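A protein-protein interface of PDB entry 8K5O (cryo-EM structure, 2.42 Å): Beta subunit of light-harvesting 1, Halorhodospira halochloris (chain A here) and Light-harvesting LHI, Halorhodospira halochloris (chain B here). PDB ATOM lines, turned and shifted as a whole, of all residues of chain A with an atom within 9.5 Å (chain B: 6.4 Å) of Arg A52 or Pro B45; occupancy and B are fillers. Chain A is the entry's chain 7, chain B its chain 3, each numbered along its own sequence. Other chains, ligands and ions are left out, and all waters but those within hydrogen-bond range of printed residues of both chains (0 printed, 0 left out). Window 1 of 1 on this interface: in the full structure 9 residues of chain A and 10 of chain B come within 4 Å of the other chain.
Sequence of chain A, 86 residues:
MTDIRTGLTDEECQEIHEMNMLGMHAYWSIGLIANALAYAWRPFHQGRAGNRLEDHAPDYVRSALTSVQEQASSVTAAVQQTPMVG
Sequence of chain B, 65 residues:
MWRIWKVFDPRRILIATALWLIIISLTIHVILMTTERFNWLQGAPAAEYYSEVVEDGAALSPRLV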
ATOM      1  N   HIS A  45      37.486   0.145 -19.425  1.00  0.00           N
ATOM      2  CA  HIS A  45      36.673  -0.640 -18.515  1.00  0.00           C
ATOM      3  C   HIS A  45      36.163   0.277 -17.417  1.00  0.00           C
ATOM      4  O   HIS A  45      36.947   0.986 -16.781  1.00  0.00           O
ATOM      5  CB  HIS A  45      37.502  -1.792 -17.959  1.00  0.00           C
ATOM      6  CG  HIS A  45      38.305  -2.488 -19.011  1.00  0.00           C
ATOM      7  ND1 HIS A  45      39.632  -2.195 -19.240  1.00  0.00           N
ATOM      8  CD2 HIS A  45      37.951  -3.386 -19.958  1.00  0.00           C
ATOM      9  CE1 HIS A  45      40.075  -2.925 -20.246  1.00  0.00           C
ATOM     10  NE2 HIS A  45      39.074  -3.656 -20.700  1.00  0.00           N
ATOM     11  N   GLN A  46      34.851   0.286 -17.220  1.00  0.00           N
ATOM     12  CA  GLN A  46      34.260   1.218 -16.278  1.00  0.00           C
ATOM     13  C   GLN A  46      34.512   0.765 -14.846  1.00  0.00           C
ATOM     14  O   GLN A  46      34.675  -0.422 -14.555  1.00  0.00           O
ATOM     15  CB  GLN A  46      32.761   1.364 -16.540  1.00  0.00           C
ATOM     16  CG  GLN A  46      31.938   0.132 -16.245  1.00  0.00           C
ATOM     17  CD  GLN A  46      31.880  -0.829 -17.408  1.00  0.00           C
ATOM     18  OE1 GLN A  46      32.840  -0.969 -18.158  1.00  0.00           O
ATOM     19  NE2 GLN A  46      30.748  -1.495 -17.567  1.00  0.00           N
ATOM     20  N   GLY A  47      34.557   1.739 -13.945  1.00  0.00           N
ATOM     21  CA  GLY A  47      34.600   1.449 -12.534  1.00  0.00           C
ATOM     22  C   GLY A  47      33.249   1.001 -12.037  1.00  0.00           C
ATOM     23  O   GLY A  47      32.270   0.925 -12.780  1.00  0.00           O
ATOM     24  N   ARG A  48      33.201   0.694 -10.742  1.00  0.00           N
ATOM     25  CA  ARG A  48      31.958   0.227 -10.143  1.00  0.00           C
ATOM     26  C   ARG A  48      30.834   1.234 -10.354  1.00  0.00           C
ATOM     27  O   ARG A  48      29.676   0.850 -10.553  1.00  0.00           O
ATOM     28  CB  ARG A  48      32.177  -0.059  -8.659  1.00  0.00           C
ATOM     29  CG  ARG A  48      33.184  -1.162  -8.418  1.00  0.00           C
ATOM     30  CD  ARG A  48      32.594  -2.498  -8.813  1.00  0.00           C
ATOM     31  NE  ARG A  48      33.570  -3.581  -8.779  1.00  0.00           N
ATOM     32  CZ  ARG A  48      33.877  -4.285  -7.698  1.00  0.00           C
ATOM     33  NH1 ARG A  48      33.348  -4.007  -6.518  1.00  0.00           N
ATOM     34  NH2 ARG A  48      34.742  -5.288  -7.804  1.00  0.00           N
ATOM     35  N   ALA A  49      31.162   2.526 -10.346  1.00  0.00           N
ATOM     36  CA  ALA A  49      30.192   3.566 -10.661  1.00  0.00           C
ATOM     37  C   ALA A  49      29.796   3.577 -12.128  1.00  0.00           C
ATOM     38  O   ALA A  49      28.836   4.267 -12.485  1.00  0.00           O
ATOM     39  CB  ALA A  49      30.751   4.935 -10.280  1.00  0.00           C
ATOM     40  N   GLY A  50      30.508   2.849 -12.979  1.00  0.00           N
ATOM     41  CA  GLY A  50      30.275   2.917 -14.402  1.00  0.00           C
ATOM     42  C   GLY A  50      30.852   4.185 -14.990  1.00  0.00           C
ATOM     43  O   GLY A  50      31.456   5.015 -14.311  1.00  0.00           O
ATOM     44  N   ASN A  51      30.666   4.333 -16.297  1.00  0.00           N
ATOM     45  CA  ASN A  51      31.026   5.575 -16.962  1.00  0.00           C
ATOM     46  C   ASN A  51      29.958   5.982 -17.963  1.00  0.00           C
ATOM     47  O   ASN A  51      30.262   6.606 -18.984  1.00  0.00           O
ATOM     48  CB  ASN A  51      32.397   5.482 -17.641  1.00  0.00           C
ATOM     49  CG  ASN A  51      32.559   4.233 -18.476  1.00  0.00           C
ATOM     50  OD1 ASN A  51      31.616   3.759 -19.099  1.00  0.00           O
ATOM     51  ND2 ASN A  51      33.769   3.697 -18.497  1.00  0.00           N
ATOM     52  N   ARG A  52      28.707   5.627 -17.689  1.00  0.00           N
ATOM     53  CA  ARG A  52      27.599   6.118 -18.492  1.00  0.00           C
ATOM     54  C   ARG A  52      27.394   7.602 -18.229  1.00  0.00           C
ATOM     55  O   ARG A  52      27.431   8.057 -17.083  1.00  0.00           O
ATOM     56  CB  ARG A  52      26.323   5.341 -18.173  1.00  0.00           C
ATOM     57  CG  ARG A  52      26.236   4.004 -18.874  1.00  0.00           C
ATOM     58  CD  ARG A  52      24.987   3.234 -18.509  1.00  0.00           C
ATOM     59  NE  ARG A  52      24.526   3.530 -17.160  1.00  0.00           N
ATOM     60  CZ  ARG A  52      23.420   3.031 -16.626  1.00  0.00           C
ATOM     61  NH1 ARG A  52      22.643   2.199 -17.297  1.00  0.00           N
ATOM     62  NH2 ARG A  52      23.084   3.381 -15.389  1.00  0.00           N
ATOM     63  N   LEU A  53      27.185   8.362 -19.305  1.00  0.00           N
ATOM     64  CA  LEU A  53      26.999   9.801 -19.163  1.00  0.00           C
ATOM     65  C   LEU A  53      25.763  10.112 -18.334  1.00  0.00           C
ATOM     66  O   LEU A  53      25.773  11.037 -17.515  1.00  0.00           O
ATOM     67  CB  LEU A  53      26.891  10.457 -20.538  1.00  0.00           C
ATOM     68  CG  LEU A  53      28.184  10.938 -21.190  1.00  0.00           C
ATOM     69  CD1 LEU A  53      27.860  11.689 -22.468  1.00  0.00           C
ATOM     70  CD2 LEU A  53      28.983  11.806 -20.237  1.00  0.00           C
ATOM     71  N   GLU A  54      24.696   9.337 -18.522  1.00  0.00           N
ATOM     72  CA  GLU A  54      23.439   9.602 -17.833  1.00  0.00           C
ATOM     73  C   GLU A  54      23.590   9.551 -16.318  1.00  0.00           C
ATOM     74  O   GLU A  54      22.852  10.236 -15.601  1.00  0.00           O
ATOM     75  CB  GLU A  54      22.384   8.606 -18.303  1.00  0.00           C
ATOM     76  CG  GLU A  54      22.730   7.162 -18.003  1.00  0.00           C
ATOM     77  CD  GLU A  54      21.710   6.200 -18.558  1.00  0.00           C
ATOM     78  OE1 GLU A  54      20.739   6.661 -19.190  1.00  0.00           O
ATOM     79  OE2 GLU A  54      21.874   4.982 -18.366  1.00  0.00           O
ATOM     80  N   ASP A  55      24.529   8.757 -15.810  1.00  0.00           N
ATOM     81  CA  ASP A  55      24.723   8.645 -14.372  1.00  0.00           C
ATOM     82  C   ASP A  55      25.615   9.733 -13.796  1.00  0.00           C
ATOM     83  O   ASP A  55      25.664   9.881 -12.572  1.00  0.00           O
ATOM     84  CB  ASP A  55      25.315   7.281 -14.022  1.00  0.00           C
ATOM     85  CG  ASP A  55      24.437   6.134 -14.463  1.00  0.00           C
ATOM     86  OD1 ASP A  55      23.205   6.224 -14.290  1.00  0.00           O
ATOM     87  OD2 ASP A  55      24.979   5.141 -14.984  1.00  0.00           O
ATOM     88  N   HIS A  56      26.316  10.496 -14.631  1.00  0.00           N
ATOM     89  CA  HIS A  56      27.291  11.444 -14.110  1.00  0.00           C
ATOM     90  C   HIS A  56      27.101  12.844 -14.676  1.00  0.00           C
ATOM     91  O   HIS A  56      27.395  13.833 -13.999  1.00  0.00           O
ATOM     92  CB  HIS A  56      28.704  10.934 -14.391  1.00  0.00           C
ATOM     93  CG  HIS A  56      28.955   9.556 -13.866  1.00  0.00           C
ATOM     94  ND1 HIS A  56      28.835   8.427 -14.645  1.00  0.00           N
ATOM     95  CD2 HIS A  56      29.297   9.124 -12.629  1.00  0.00           C
ATOM     96  CE1 HIS A  56      29.103   7.360 -13.914  1.00  0.00           C
ATOM     97  NE2 HIS A  56      29.387   7.755 -12.688  1.00  0.00           N
ATOM     98  N   ALA A  57      26.611  12.941 -15.906  1.00  0.00           N
ATOM     99  CA  ALA A  57      26.393  14.238 -16.521  1.00  0.00           C
ATOM    100  C   ALA A  57      25.202  14.944 -15.868  1.00  0.00           C
ATOM    101  O   ALA A  57      24.318  14.295 -15.305  1.00  0.00           O
ATOM    102  CB  ALA A  57      26.161  14.078 -18.019  1.00  0.00           C
ATOM    103  N   PRO A  58      25.158  16.285 -15.925  1.00  0.00           N
ATOM    104  CA  PRO A  58      24.135  17.020 -15.166  1.00  0.00           C
ATOM    105  C   PRO A  58      22.767  17.085 -15.828  1.00  0.00           C
ATOM    106  O   PRO A  58      22.151  18.153 -15.871  1.00  0.00           O
ATOM    107  CB  PRO A  58      24.741  18.428 -15.038  1.00  0.00           C
ATOM    108  CG  PRO A  58      26.162  18.310 -15.498  1.00  0.00           C
ATOM    109  CD  PRO A  58      26.174  17.193 -16.473  1.00  0.00           C
ATOM    110  N   ASP A  59      22.283  15.961 -16.350  1.00  0.00           N
ATOM    111  CA  ASP A  59      20.899  15.739 -16.763  1.00  0.00           C
ATOM    112  C   ASP A  59      20.466  16.565 -17.966  1.00  0.00           C
ATOM    113  O   ASP A  59      19.356  16.357 -18.466  1.00  0.00           O
ATOM    114  CB  ASP A  59      19.902  15.997 -15.623  1.00  0.00           C
ATOM    115  CG  ASP A  59      19.995  14.963 -14.519  1.00  0.00           C
ATOM    116  OD1 ASP A  59      20.364  13.806 -14.813  1.00  0.00           O
ATOM    117  OD2 ASP A  59      19.697  15.307 -13.357  1.00  0.00           O
ATOM    118  N   VAL A  61      23.058  17.032 -20.461  1.00  0.00           N
ATOM    119  CA  VAL A  61      23.933  16.406 -21.443  1.00  0.00           C
ATOM    120  C   VAL A  61      23.214  15.184 -21.996  1.00  0.00           C
ATOM    121  O   VAL A  61      22.917  14.240 -21.256  1.00  0.00           O
ATOM    122  CB  VAL A  61      25.278  16.021 -20.815  1.00  0.00           C
ATOM    123  CG1 VAL A  61      26.210  15.436 -21.859  1.00  0.00           C
ATOM    124  CG2 VAL A  61      25.904  17.224 -20.134  1.00  0.00           C
ATOM    125  N   ARG A  62      22.922  15.205 -23.291  1.00  0.00           N
ATOM    126  CA  ARG A  62      22.228  14.091 -23.914  1.00  0.00           C
ATOM    127  C   ARG A  62      23.116  12.856 -23.940  1.00  0.00           C
ATOM    128  O   ARG A  62      24.319  12.939 -24.195  1.00  0.00           O
ATOM    129  CB  ARG A  62      21.799  14.457 -25.331  1.00  0.00           C
ATOM    130  CG  ARG A  62      20.839  13.467 -25.954  1.00  0.00           C
ATOM    131  CD  ARG A  62      20.819  13.592 -27.463  1.00  0.00           C
ATOM    132  NE  ARG A  62      22.157  13.686 -28.030  1.00  0.00           N
ATOM    133  CZ  ARG A  62      22.714  12.750 -28.785  1.00  0.00           C
ATOM    134  NH1 ARG A  62      22.081  11.625 -29.067  1.00  0.00           N
ATOM    135  NH2 ARG A  62      23.933  12.952 -29.274  1.00  0.00           N
ATOM    136  N   SER A  63      22.513  11.705 -23.666  1.00  0.00           N
ATOM    137  CA  SER A  63      23.201  10.425 -23.725  1.00  0.00           C
ATOM    138  C   SER A  63      22.566   9.578 -24.815  1.00  0.00           C
ATOM    139  O   SER A  63      21.343   9.408 -24.841  1.00  0.00           O
ATOM    140  CB  SER A  63      23.144   9.698 -22.379  1.00  0.00           C
ATOM    141  OG  SER A  63      24.027   8.591 -22.362  1.00  0.00           O
ATOM    142  N   ALA A  64      23.398   9.062 -25.721  1.00  0.00           N
ATOM    143  CA  ALA A  64      22.894   8.173 -26.759  1.00  0.00           C
ATOM    144  C   ALA A  64      22.385   6.868 -26.164  1.00  0.00           C
ATOM    145  O   ALA A  64      21.498   6.222 -26.730  1.00  0.00           O
ATOM    146  CB  ALA A  64      23.983   7.905 -27.796  1.00  0.00           C
ATOM    147  N   LEU A  65      22.936   6.468 -25.024  1.00  0.00           N
ATOM    148  CA  LEU A  65      22.547   5.234 -24.361  1.00  0.00           C
ATOM    149  C   LEU A  65      21.112   5.300 -23.857  1.00  0.00           C
ATOM    150  O   LEU A  65      20.436   4.278 -23.745  1.00  0.00           O
ATOM    151  CB  LEU A  65      23.497   4.941 -23.202  1.00  0.00           C
ATOM    152  CG  LEU A  65      24.946   4.696 -23.616  1.00  0.00           C
ATOM    153  CD1 LEU A  65      25.836   4.566 -22.398  1.00  0.00           C
ATOM    154  CD2 LEU A  65      25.050   3.467 -24.498  1.00  0.00           C
ATOM    155  N   GLU B  36      24.628  -6.089 -19.205  1.00  0.00           N
ATOM    156  CA  GLU B  36      24.707  -4.774 -18.593  1.00  0.00           C
ATOM    157  C   GLU B  36      25.943  -4.619 -17.726  1.00  0.00           C
ATOM    158  O   GLU B  36      26.591  -3.570 -17.754  1.00  0.00           O
ATOM    159  CB  GLU B  36      23.461  -4.511 -17.748  1.00  0.00           C
ATOM    160  CG  GLU B  36      23.415  -3.132 -17.140  1.00  0.00           C
ATOM    161  CD  GLU B  36      22.207  -2.927 -16.264  1.00  0.00           C
ATOM    162  OE1 GLU B  36      21.445  -3.895 -16.077  1.00  0.00           O
ATOM    163  OE2 GLU B  36      22.025  -1.803 -15.754  1.00  0.00           O
ATOM    164  N   ARG B  37      26.296  -5.655 -16.969  1.00  0.00           N
ATOM    165  CA  ARG B  37      27.421  -5.536 -16.055  1.00  0.00           C
ATOM    166  C   ARG B  37      28.742  -5.577 -16.803  1.00  0.00           C
ATOM    167  O   ARG B  37      29.689  -4.868 -16.448  1.00  0.00           O
ATOM    168  CB  ARG B  37      27.378  -6.656 -15.028  1.00  0.00           C
ATOM    169  CG  ARG B  37      28.522  -6.632 -14.050  1.00  0.00           C
ATOM    170  CD  ARG B  37      28.442  -7.871 -13.251  1.00  0.00           C
ATOM    171  NE  ARG B  37      29.468  -8.096 -12.247  1.00  0.00           N
ATOM    172  CZ  ARG B  37      29.463  -7.541 -11.044  1.00  0.00           C
ATOM    173  NH1 ARG B  37      28.514  -6.699 -10.674  1.00  0.00           N
ATOM    174  NH2 ARG B  37      30.420  -7.860 -10.182  1.00  0.00           N
ATOM    175  N   GLN B  42      29.152  -0.050 -23.187  1.00  0.00           N
ATOM    176  CA  GLN B  42      28.046   0.698 -22.602  1.00  0.00           C
ATOM    177  C   GLN B  42      28.449   1.334 -21.276  1.00  0.00           C
ATOM    178  O   GLN B  42      27.990   2.432 -20.943  1.00  0.00           O
ATOM    179  CB  GLN B  42      26.840  -0.220 -22.420  1.00  0.00           C
ATOM    180  CG  GLN B  42      25.622   0.452 -21.818  1.00  0.00           C
ATOM    181  CD  GLN B  42      24.840  -0.468 -20.904  1.00  0.00           C
ATOM    182  OE1 GLN B  42      25.045  -1.682 -20.898  1.00  0.00           O
ATOM    183  NE2 GLN B  42      23.944   0.109 -20.113  1.00  0.00           N
ATOM    184  N   GLY B  43      29.304   0.665 -20.513  1.00  0.00           N
ATOM    185  CA  GLY B  43      29.821   1.217 -19.273  1.00  0.00           C
ATOM    186  C   GLY B  43      28.826   1.371 -18.142  1.00  0.00           C
ATOM    187  O   GLY B  43      28.887   2.361 -17.404  1.00  0.00           O
ATOM    188  N   ALA B  44      27.929   0.407 -17.969  1.00  0.00           N
ATOM    189  CA  ALA B  44      26.941   0.495 -16.908  1.00  0.00           C
ATOM    190  C   ALA B  44      27.590   0.265 -15.544  1.00  0.00           C
ATOM    191  O   ALA B  44      28.617  -0.408 -15.443  1.00  0.00           O
ATOM    192  CB  ALA B  44      25.826  -0.520 -17.134  1.00  0.00           C
ATOM    193  N   PRO B  45      27.012   0.818 -14.481  1.00  0.00           N
ATOM    194  CA  PRO B  45      27.565   0.602 -13.141  1.00  0.00           C
ATOM    195  C   PRO B  45      27.424  -0.843 -12.693  1.00  0.00           C
ATOM    196  O   PRO B  45      26.585  -1.605 -13.179  1.00  0.00           O
ATOM    197  CB  PRO B  45      26.733   1.529 -12.251  1.00  0.00           C
ATOM    198  CG  PRO B  45      26.026   2.446 -13.175  1.00  0.00           C
ATOM    199  CD  PRO B  45      25.853   1.721 -14.457  1.00  0.00           C
ATOM    200  N   ALA B  46      28.278  -1.217 -11.752  1.00  0.00           N
ATOM    201  CA  ALA B  46      28.216  -2.530 -11.137  1.00  0.00           C
ATOM    202  C   ALA B  46      27.344  -2.490  -9.889  1.00  0.00           C
ATOM    203  O   ALA B  46      27.235  -1.470  -9.207  1.00  0.00           O
ATOM    204  CB  ALA B  46      29.615  -3.030 -10.783  1.00  0.00           C
ATOM    205  N   ALA B  47      26.720  -3.629  -9.594  1.00  0.00           N
ATOM    206  CA  ALA B  47      25.855  -3.726  -8.426  1.00  0.00           C
ATOM    207  C   ALA B  47      26.620  -3.580  -7.120  1.00  0.00           C
ATOM    208  O   ALA B  47      26.016  -3.217  -6.107  1.00  0.00           O
ATOM    209  CB  ALA B  47      25.107  -5.055  -8.441  1.00  0.00           C
ATOM    210  N   GLU B  48      27.926  -3.856  -7.113  1.00  0.00           N
ATOM    211  CA  GLU B  48      28.713  -3.686  -5.896  1.00  0.00           C
ATOM    212  C   GLU B  48      28.788  -2.225  -5.480  1.00  0.00           C
ATOM    213  O   GLU B  48      28.969  -1.923  -4.295  1.00  0.00           O
ATOM    214  CB  GLU B  48      30.119  -4.245  -6.099  1.00  0.00           C
ATOM    215  CG  GLU B  48      30.193  -5.755  -6.128  1.00  0.00           C
ATOM    216  CD  GLU B  48      30.022  -6.317  -7.522  1.00  0.00           C
ATOM    217  OE1 GLU B  48      29.225  -5.755  -8.300  1.00  0.00           O
ATOM    218  OE2 GLU B  48      30.685  -7.325  -7.842  1.00  0.00           O
ATOM    219  N   TYR B  49      28.664  -1.311  -6.437  1.00  0.00           N
ATOM    220  CA  TYR B  49      28.681   0.114  -6.155  1.00  0.00           C
ATOM    221  C   TYR B  49      27.379   0.607  -5.538  1.00  0.00           C
ATOM    222  O   TYR B  49      27.403   1.590  -4.791  1.00  0.00           O
ATOM    223  CB  TYR B  49      28.968   0.873  -7.450  1.00  0.00           C
ATOM    224  CG  TYR B  49      29.191   2.355  -7.296  1.00  0.00           C
ATOM    225  CD1 TYR B  49      30.432   2.855  -6.937  1.00  0.00           C
ATOM    226  CD2 TYR B  49      28.170   3.256  -7.541  1.00  0.00           C
ATOM    227  CE1 TYR B  49      30.640   4.209  -6.805  1.00  0.00           C
ATOM    228  CE2 TYR B  49      28.368   4.608  -7.412  1.00  0.00           C
ATOM    229  CZ  TYR B  49      29.604   5.082  -7.043  1.00  0.00           C
ATOM    230  OH  TYR B  49      29.806   6.434  -6.915  1.00  0.00           O
ATOM    231  N   SER B  51      24.778   1.832  -7.407  1.00  0.00           N
ATOM    232  CA  SER B  51      24.822   3.081  -8.170  1.00  0.00           C
ATOM    233  C   SER B  51      23.797   4.122  -7.752  1.00  0.00           C
ATOM    234  O   SER B  51      23.945   5.303  -8.062  1.00  0.00           O
ATOM    235  CB  SER B  51      24.646   2.786  -9.657  1.00  0.00           C
ATOM    236  OG  SER B  51      24.972   3.925 -10.433  1.00  0.00           O
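The backbone carbonyl oxygen (O) of Gly B43 lies within hydrogen-bond range of the backbone NH (N) of Asn A51. The backbone NH (N) of Arg A52 is in hydrogen-bond range of the backbone carbonyl oxygen (O) of Gly B43 (3.3 Å). The backbone carbonyl oxygen (O) of Ala B44 sits at hydrogen-bond distance from the side-chain amide nitrogen (NE2) of Gln A46, 3.2 Å away. O of Arg A48 lies within hydrogen-bond range of N of Ala B46 (2.8 Å).
Hydrophobic or aromatic side chains of chain B that line the printed part of chain A: Pro B45, Ala B46 and Tyr B49. Along chain B the printed residues that touch a printed residue of chain A span positions 37 to 49. Among the printed residues, no Asp or Glu carboxylate lies within 4 Å of a Lys or Arg side-chain nitrogen of the other chain.
The guanidinium group (NH2) of Arg B37 lies within salt-bridge range of the side-chain carboxylate (OE2) of Glu B48 (2.4 Å). The guanidinium group (NH1) of Arg A52 lies within salt-bridge range of the side-chain carboxylate (OE2) of Glu A54 (3.1 Å). NH2 of Arg A52 is in salt-bridge range of OD2 of Asp A55, 2.6 Å away. A ring nitrogen (ND1) of His A56 lies within hydrogen-bond range of the backbone carbonyl oxygen (O) of Arg A52 (2.8 Å).
Arg B37 touches Gln A46. Glu B48 touches Arg A48 (CB to NH1, 3.3 Å). Arg A48 touches Tyr B49. CG of Pro B45 touches O of Ala A49, 3.4 Å away. O of Gly B43 touches CA of Gly A50 (3.4 Å). Gly A50 touches Ala B44 (CA to O, 3.9 Å). N of Gly A50 touches CA of Pro B45, 3.7 Å away. Arg A52 touches Gln B42. CA of Ala B44 touches CD of Arg A52, 3.7 Å away. O of Gln B42 touches CD1 of Leu A65, at 3.4 Å.
Of chain B, only Gln B42 (3.1 Å), Gly B43 (3.3 Å), Ala B44 (3.7 Å) and Pro B45 (3.4 Å) come within 4 Å of Arg A52. Pro B45 touches five residues of chain A. Gly B43 touches four residues of chain A. Of the printed residues of chain A, Ala B44 touches Gln A46 (3.2 Å), Gly A50 (3.9 Å) and Arg A52 (3.7 Å). Of the printed residues of chain B, Gln A46 touches Arg B37, Gly B43 and Ala B44. Of the printed residues of chain B, Leu A65 touches Gln B42 (3.4 Å). Printed residues of chain B within 4 Å of Asn A51: Gly B43 (2.9 Å). Printed residues of chain B within 4 Å of Arg A48: Pro B45, Ala B46, Glu B48 and Tyr B49. Ala B47 touches none of the printed residues of chain A. The nearest residue of chain A that does not touch Pro B45 is Gly A47 (4.7 Å). The nearest printed residue of chain B that does not touch Ala A49 is Ser B51 (4.4 Å).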
